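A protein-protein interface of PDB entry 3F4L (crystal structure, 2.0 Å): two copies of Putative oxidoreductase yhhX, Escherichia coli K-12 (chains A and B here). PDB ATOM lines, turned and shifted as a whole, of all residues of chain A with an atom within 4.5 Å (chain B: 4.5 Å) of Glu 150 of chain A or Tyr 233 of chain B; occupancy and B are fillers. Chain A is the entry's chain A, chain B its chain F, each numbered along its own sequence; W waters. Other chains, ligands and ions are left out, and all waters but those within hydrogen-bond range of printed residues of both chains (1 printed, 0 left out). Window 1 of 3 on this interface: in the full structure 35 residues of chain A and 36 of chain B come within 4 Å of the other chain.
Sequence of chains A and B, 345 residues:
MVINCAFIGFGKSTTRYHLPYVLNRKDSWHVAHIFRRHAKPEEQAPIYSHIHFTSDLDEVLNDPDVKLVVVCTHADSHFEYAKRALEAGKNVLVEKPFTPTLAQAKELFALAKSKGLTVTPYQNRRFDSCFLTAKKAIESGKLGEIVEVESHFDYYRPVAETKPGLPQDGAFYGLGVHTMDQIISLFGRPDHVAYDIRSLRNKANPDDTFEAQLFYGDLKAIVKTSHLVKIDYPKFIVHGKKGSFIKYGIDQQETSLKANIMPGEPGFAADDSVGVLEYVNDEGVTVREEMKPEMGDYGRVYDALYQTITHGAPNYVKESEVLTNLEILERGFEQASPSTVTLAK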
ATOM      1  N   GLU A 148      -0.511 -17.959  13.415  1.00  0.00           N
ATOM      2  CA  GLU A 148       0.339 -17.907  14.588  1.00  0.00           C
ATOM      3  C   GLU A 148       1.639 -17.136  14.380  1.00  0.00           C
ATOM      4  O   GLU A 148       2.282 -17.231  13.337  1.00  0.00           O
ATOM      5  CB  GLU A 148       0.650 -19.319  15.099  1.00  0.00           C
ATOM      6  CG  GLU A 148       1.277 -19.317  16.497  1.00  0.00           C
ATOM      7  CD  GLU A 148       0.872 -20.520  17.345  1.00  0.00           C
ATOM      8  OE1 GLU A 148      -0.334 -20.839  17.385  1.00  0.00           O
ATOM      9  OE2 GLU A 148       1.754 -21.131  17.987  1.00  0.00           O
ATOM     10  N   VAL A 149       1.991 -16.357  15.394  1.00  0.00           N
ATOM     11  CA  VAL A 149       3.206 -15.557  15.396  1.00  0.00           C
ATOM     12  C   VAL A 149       3.850 -15.833  16.749  1.00  0.00           C
ATOM     13  O   VAL A 149       3.163 -15.903  17.773  1.00  0.00           O
ATOM     14  CB  VAL A 149       2.887 -14.039  15.246  1.00  0.00           C
ATOM     15  CG1 VAL A 149       4.168 -13.193  15.397  1.00  0.00           C
ATOM     16  CG2 VAL A 149       2.271 -13.773  13.882  1.00  0.00           C
ATOM     17  N   GLU A 150       5.163 -16.027  16.753  1.00  0.00           N
ATOM     18  CA  GLU A 150       5.865 -16.296  17.993  1.00  0.00           C
ATOM     19  C   GLU A 150       7.121 -15.433  18.020  1.00  0.00           C
ATOM     20  O   GLU A 150       7.925 -15.469  17.091  1.00  0.00           O
ATOM     21  CB  GLU A 150       6.228 -17.778  18.071  1.00  0.00           C
ATOM     22  CG  GLU A 150       6.619 -18.277  19.460  1.00  0.00           C
ATOM     23  CD  GLU A 150       6.799 -19.796  19.503  1.00  0.00           C
ATOM     24  OE1 GLU A 150       5.910 -20.526  19.011  1.00  0.00           O
ATOM     25  OE2 GLU A 150       7.828 -20.265  20.036  1.00  0.00           O
ATOM     26  N   SER A 151       7.265 -14.647  19.081  1.00  0.00           N
ATOM     27  CA  SER A 151       8.411 -13.763  19.254  1.00  0.00           C
ATOM     28  C   SER A 151       9.189 -14.123  20.522  1.00  0.00           C
ATOM     29  O   SER A 151       8.603 -14.287  21.596  1.00  0.00           O
ATOM     30  CB  SER A 151       7.934 -12.315  19.340  1.00  0.00           C
ATOM     31  OG  SER A 151       8.999 -11.449  19.669  1.00  0.00           O
ATOM     32  N   HIS A 152      10.508 -14.238  20.394  1.00  0.00           N
ATOM     33  CA  HIS A 152      11.365 -14.572  21.523  1.00  0.00           C
ATOM     34  C   HIS A 152      12.417 -13.492  21.744  1.00  0.00           C
ATOM     35  O   HIS A 152      12.964 -12.934  20.798  1.00  0.00           O
ATOM     36  CB  HIS A 152      12.093 -15.906  21.296  1.00  0.00           C
ATOM     37  CG  HIS A 152      11.264 -17.123  21.581  1.00  0.00           C
ATOM     38  ND1 HIS A 152      10.395 -17.673  20.662  1.00  0.00           N
ATOM     39  CD2 HIS A 152      11.189 -17.907  22.683  1.00  0.00           C
ATOM     40  CE1 HIS A 152       9.823 -18.744  21.185  1.00  0.00           C
ATOM     41  NE2 HIS A 152      10.287 -18.907  22.412  1.00  0.00           N
ATOM     42  N   ILE A 222       2.309 -14.907  20.144  1.00  0.00           N
ATOM     43  CA  ILE A 222       3.016 -15.215  21.377  1.00  0.00           C
ATOM     44  C   ILE A 222       4.281 -14.374  21.556  1.00  0.00           C
ATOM     45  O   ILE A 222       5.103 -14.262  20.649  1.00  0.00           O
ATOM     46  CB  ILE A 222       3.390 -16.709  21.392  1.00  0.00           C
ATOM     47  CG1 ILE A 222       2.107 -17.549  21.470  1.00  0.00           C
ATOM     48  CG2 ILE A 222       4.318 -17.011  22.555  1.00  0.00           C
ATOM     49  CD1 ILE A 222       2.338 -19.053  21.357  1.00  0.00           C
ATOM     50  N   LYS A 235      14.178 -16.155  16.439  1.00  0.00           N
ATOM     51  CA  LYS A 235      13.755 -14.839  16.926  1.00  0.00           C
ATOM     52  C   LYS A 235      12.256 -14.632  16.625  1.00  0.00           C
ATOM     53  O   LYS A 235      11.513 -14.084  17.441  1.00  0.00           O
ATOM     54  CB  LYS A 235      14.576 -13.735  16.251  1.00  0.00           C
ATOM     55  CG  LYS A 235      14.161 -12.323  16.662  1.00  0.00           C
ATOM     56  CD  LYS A 235      14.554 -12.008  18.104  1.00  0.00           C
ATOM     57  CE  LYS A 235      13.785 -10.795  18.643  1.00  0.00           C
ATOM     58  NZ  LYS A 235      12.323 -11.103  18.743  1.00  0.00           N
ATOM     59  N   PHE A 236      11.832 -15.056  15.438  1.00  0.00           N
ATOM     60  CA  PHE A 236      10.422 -14.962  15.045  1.00  0.00           C
ATOM     61  C   PHE A 236      10.001 -16.212  14.297  1.00  0.00           C
ATOM     62  O   PHE A 236      10.786 -16.804  13.538  1.00  0.00           O
ATOM     63  CB  PHE A 236      10.144 -13.775  14.108  1.00  0.00           C
ATOM     64  CG  PHE A 236      10.179 -12.433  14.778  1.00  0.00           C
ATOM     65  CD1 PHE A 236      11.306 -11.618  14.671  1.00  0.00           C
ATOM     66  CD2 PHE A 236       9.090 -11.984  15.518  1.00  0.00           C
ATOM     67  CE1 PHE A 236      11.349 -10.372  15.298  1.00  0.00           C
ATOM     68  CE2 PHE A 236       9.120 -10.739  16.145  1.00  0.00           C
ATOM     69  CZ  PHE A 236      10.249  -9.932  16.036  1.00  0.00           C
ATOM     70  N   ILE A 237       8.747 -16.593  14.504  1.00  0.00           N
ATOM     71  CA  ILE A 237       8.154 -17.737  13.828  1.00  0.00           C
ATOM     72  C   ILE A 237       6.782 -17.236  13.400  1.00  0.00           C
ATOM     73  O   ILE A 237       6.083 -16.615  14.195  1.00  0.00           O
ATOM     74  CB  ILE A 237       7.937 -18.938  14.770  1.00  0.00           C
ATOM     75  CG1 ILE A 237       9.276 -19.475  15.272  1.00  0.00           C
ATOM     76  CG2 ILE A 237       7.188 -20.046  14.023  1.00  0.00           C
ATOM     77  CD1 ILE A 237       9.124 -20.648  16.212  1.00  0.00           C
ATOM     78  N   HIS A 239       3.316 -18.633  11.160  1.00  0.00           N
ATOM     79  CA  HIS A 239       2.677 -19.730  10.443  1.00  0.00           C
ATOM     80  C   HIS A 239       1.370 -19.225   9.864  1.00  0.00           C
ATOM     81  O   HIS A 239       0.578 -18.604  10.569  1.00  0.00           O
ATOM     82  CB  HIS A 239       2.401 -20.925  11.383  1.00  0.00           C
ATOM     83  CG  HIS A 239       3.639 -21.653  11.807  1.00  0.00           C
ATOM     84  ND1 HIS A 239       4.507 -22.232  10.907  1.00  0.00           N
ATOM     85  CD2 HIS A 239       4.173 -21.869  13.033  1.00  0.00           C
ATOM     86  CE1 HIS A 239       5.523 -22.768  11.557  1.00  0.00           C
ATOM     87  NE2 HIS A 239       5.345 -22.561  12.850  1.00  0.00           N
ATOM     88  N   HIS B 152       5.794 -30.810  20.581  1.00  0.00           N
ATOM     89  CA  HIS B 152       5.027 -30.520  19.376  1.00  0.00           C
ATOM     90  C   HIS B 152       4.608 -31.777  18.619  1.00  0.00           C
ATOM     91  O   HIS B 152       5.379 -32.731  18.504  1.00  0.00           O
ATOM     92  CB  HIS B 152       5.846 -29.658  18.410  1.00  0.00           C
ATOM     93  CG  HIS B 152       5.771 -28.192  18.683  1.00  0.00           C
ATOM     94  ND1 HIS B 152       6.599 -27.557  19.583  1.00  0.00           N
ATOM     95  CD2 HIS B 152       4.949 -27.238  18.186  1.00  0.00           C
ATOM     96  CE1 HIS B 152       6.289 -26.274  19.631  1.00  0.00           C
ATOM     97  NE2 HIS B 152       5.291 -26.054  18.793  1.00  0.00           N
ATOM     98  N   ASP B 154       2.670 -31.834  15.121  1.00  0.00           N
ATOM     99  CA  ASP B 154       1.982 -31.123  14.060  1.00  0.00           C
ATOM    100  C   ASP B 154       2.026 -31.764  12.680  1.00  0.00           C
ATOM    101  O   ASP B 154       2.753 -32.724  12.418  1.00  0.00           O
ATOM    102  CB  ASP B 154       2.562 -29.716  13.908  1.00  0.00           C
ATOM    103  CG  ASP B 154       2.846 -29.038  15.233  1.00  0.00           C
ATOM    104  OD1 ASP B 154       1.946 -28.989  16.097  1.00  0.00           O
ATOM    105  OD2 ASP B 154       3.981 -28.535  15.393  1.00  0.00           O
ATOM    106  N   LYS B 224       1.544 -28.876  22.286  1.00  0.00           N
ATOM    107  CA  LYS B 224       0.764 -28.254  21.228  1.00  0.00           C
ATOM    108  C   LYS B 224       0.786 -28.991  19.906  1.00  0.00           C
ATOM    109  O   LYS B 224       1.747 -29.693  19.588  1.00  0.00           O
ATOM    110  CB  LYS B 224       1.201 -26.795  21.023  1.00  0.00           C
ATOM    111  CG  LYS B 224       2.698 -26.564  20.990  1.00  0.00           C
ATOM    112  CD  LYS B 224       3.024 -25.067  21.071  1.00  0.00           C
ATOM    113  CE  LYS B 224       2.359 -24.288  19.942  1.00  0.00           C
ATOM    114  NZ  LYS B 224       2.667 -22.839  19.997  1.00  0.00           N
ATOM    115  N   VAL B 229       1.360 -26.396   9.987  1.00  0.00           N
ATOM    116  CA  VAL B 229       2.770 -26.112  10.232  1.00  0.00           C
ATOM    117  C   VAL B 229       3.635 -26.595   9.068  1.00  0.00           C
ATOM    118  O   VAL B 229       3.969 -27.773   8.990  1.00  0.00           O
ATOM    119  CB  VAL B 229       3.231 -26.784  11.554  1.00  0.00           C
ATOM    120  CG1 VAL B 229       4.732 -26.554  11.784  1.00  0.00           C
ATOM    121  CG2 VAL B 229       2.425 -26.223  12.709  1.00  0.00           C
ATOM    122  N   ILE B 231       6.850 -25.543   8.258  1.00  0.00           N
ATOM    123  CA  ILE B 231       8.222 -25.766   8.719  1.00  0.00           C
ATOM    124  C   ILE B 231       8.133 -26.212  10.177  1.00  0.00           C
ATOM    125  O   ILE B 231       7.754 -25.435  11.055  1.00  0.00           O
ATOM    126  CB  ILE B 231       9.081 -24.487   8.650  1.00  0.00           C
ATOM    127  CG1 ILE B 231       9.183 -24.000   7.209  1.00  0.00           C
ATOM    128  CG2 ILE B 231      10.501 -24.782   9.183  1.00  0.00           C
ATOM    129  CD1 ILE B 231       9.872 -22.653   7.082  1.00  0.00           C
ATOM    130  N   ASP B 232       8.487 -27.467  10.424  1.00  0.00           N
ATOM    131  CA  ASP B 232       8.399 -28.056  11.753  1.00  0.00           C
ATOM    132  C   ASP B 232       9.219 -27.432  12.867  1.00  0.00           C
ATOM    133  O   ASP B 232      10.336 -26.962  12.656  1.00  0.00           O
ATOM    134  CB  ASP B 232       8.758 -29.548  11.701  1.00  0.00           C
ATOM    135  CG  ASP B 232       7.605 -30.421  11.206  1.00  0.00           C
ATOM    136  OD1 ASP B 232       6.495 -30.332  11.770  1.00  0.00           O
ATOM    137  OD2 ASP B 232       7.813 -31.204  10.256  1.00  0.00           O
ATOM    138  N   TYR B 233       8.633 -27.441  14.061  1.00  0.00           N
ATOM    139  CA  TYR B 233       9.307 -26.969  15.258  1.00  0.00           C
ATOM    140  C   TYR B 233      10.105 -28.210  15.668  1.00  0.00           C
ATOM    141  O   TYR B 233       9.977 -29.272  15.049  1.00  0.00           O
ATOM    142  CB  TYR B 233       8.318 -26.704  16.412  1.00  0.00           C
ATOM    143  CG  TYR B 233       7.340 -25.564  16.260  1.00  0.00           C
ATOM    144  CD1 TYR B 233       6.158 -25.728  15.541  1.00  0.00           C
ATOM    145  CD2 TYR B 233       7.559 -24.345  16.899  1.00  0.00           C
ATOM    146  CE1 TYR B 233       5.207 -24.714  15.468  1.00  0.00           C
ATOM    147  CE2 TYR B 233       6.603 -23.308  16.833  1.00  0.00           C
ATOM    148  CZ  TYR B 233       5.429 -23.511  16.117  1.00  0.00           C
ATOM    149  OH  TYR B 233       4.461 -22.539  16.054  1.00  0.00           O
ATOM    150  N   PRO B 234      10.926 -28.095  16.724  1.00  0.00           N
ATOM    151  CA  PRO B 234      11.695 -29.257  17.177  1.00  0.00           C
ATOM    152  C   PRO B 234      10.642 -30.173  17.809  1.00  0.00           C
ATOM    153  O   PRO B 234       9.612 -29.679  18.262  1.00  0.00           O
ATOM    154  CB  PRO B 234      12.625 -28.660  18.234  1.00  0.00           C
ATOM    155  CG  PRO B 234      12.779 -27.219  17.790  1.00  0.00           C
ATOM    156  CD  PRO B 234      11.375 -26.864  17.404  1.00  0.00           C
ATOM    157  N   LYS B 235      10.872 -31.482  17.835  1.00  0.00           N
ATOM    158  CA  LYS B 235       9.906 -32.401  18.444  1.00  0.00           C
ATOM    159  C   LYS B 235       9.803 -32.172  19.955  1.00  0.00           C
ATOM    160  O   LYS B 235       8.711 -32.204  20.523  1.00  0.00           O
ATOM    161  CB  LYS B 235      10.304 -33.856  18.195  1.00  0.00           C
ATOM    162  CG  LYS B 235       9.342 -34.844  18.831  1.00  0.00           C
ATOM    163  CD  LYS B 235       7.959 -34.746  18.201  1.00  0.00           C
ATOM    164  CE  LYS B 235       6.901 -35.482  19.022  1.00  0.00           C
ATOM    165  NZ  LYS B 235       6.762 -34.902  20.391  1.00  0.00           N
ATOM    166  N   TYR B 248      14.961 -32.676  17.123  1.00  0.00           N
ATOM    167  CA  TYR B 248      14.157 -32.534  15.917  1.00  0.00           C
ATOM    168  C   TYR B 248      13.894 -33.945  15.422  1.00  0.00           C
ATOM    169  O   TYR B 248      14.778 -34.806  15.505  1.00  0.00           O
ATOM    170  CB  TYR B 248      14.912 -31.783  14.821  1.00  0.00           C
ATOM    171  CG  TYR B 248      14.784 -30.284  14.873  1.00  0.00           C
ATOM    172  CD1 TYR B 248      15.689 -29.513  15.602  1.00  0.00           C
ATOM    173  CD2 TYR B 248      13.771 -29.629  14.169  1.00  0.00           C
ATOM    174  CE1 TYR B 248      15.591 -28.123  15.627  1.00  0.00           C
ATOM    175  CE2 TYR B 248      13.662 -28.240  14.189  1.00  0.00           C
ATOM    176  CZ  TYR B 248      14.577 -27.493  14.921  1.00  0.00           C
ATOM    177  OH  TYR B 248      14.477 -26.118  14.960  1.00  0.00           O
HETATM  178  O   HOH W   1       7.983 -24.074  13.418  1.00  0.00           O
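The side-chain carboxylate (OE2) of Glu 148 of chain A is in salt-bridge range of the side-chain amino group (NZ) of Lys 224 of chain B (2.8 Å).
OH of Tyr 233 of chain B sits close to NE2 of His 239 of chain A, 3.3 Å away.
The backbone NH (N) of His 239 of chain A lies within hydrogen-bond range of the backbone carbonyl oxygen (O) of Glu 148 of chain A (2.8 Å).
N of Glu 150 of chain A sits at hydrogen-bond distance from O of Ile 237 of chain A (2.8 Å).
Among the printed residues, merely in contact across the chains: His 239 of chain A with Ile 231 of chain B (3.5 Å), Glu 150 of chain A with Tyr 233 of chain B (3.6 Å), Glu 148 of chain A with Tyr 233 of chain B (3.6 Å), Ile 237 of chain A with Tyr 233 of chain B (3.7 Å) and His 239 of chain A with Val 229 of chain B (3.9 Å).
Printed residues of chain B within 4 Å of Glu 148 of chain A: Lys 224 and Tyr 233.
Glu 150 of chain A touches just one residue of chain B: Tyr 233.
Printed residues of chain B within 4 Å of Ile 237 of chain A: Tyr 233.
Of the printed residues of chain A, Lys 224 of chain B touches Glu 148.
Of the printed residues of chain A, Val 229 of chain B touches His 239 (3.9 Å).
Printed residues of chain A within 4 Å of Ile 231 of chain B: His 239 (3.5 Å).
Of chain A, only Glu 148, Glu 150, Ile 237 and His 239 come within 4 Å of Tyr 233 of chain B.
The nearest printed residue of chain A that does not touch Tyr 233 of chain B is Val 149 of chain A (6.7 Å).
Printed residues of chain B that touch a printed residue of chain A: Lys 224, Val 229, Ile 231 and Tyr 233.
Hydrophobic or aromatic side chains of chain B that line the printed part of chain A: Val 229 and Tyr 233.
Hydrophobic or aromatic side chains of chain A that line the printed part of chain B: Ile 237 and His 239.
Positions printed for both chains: 152 and 235.
Of the 7 pairs that touch across the chains among the printed residues, none has its exchanged pair printed and touching as well.
Water W1 lies within hydrogen-bond range of O of Ile 231 of chain B, NE2 of His 239 of chain A and N of Tyr 233 of chain B.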
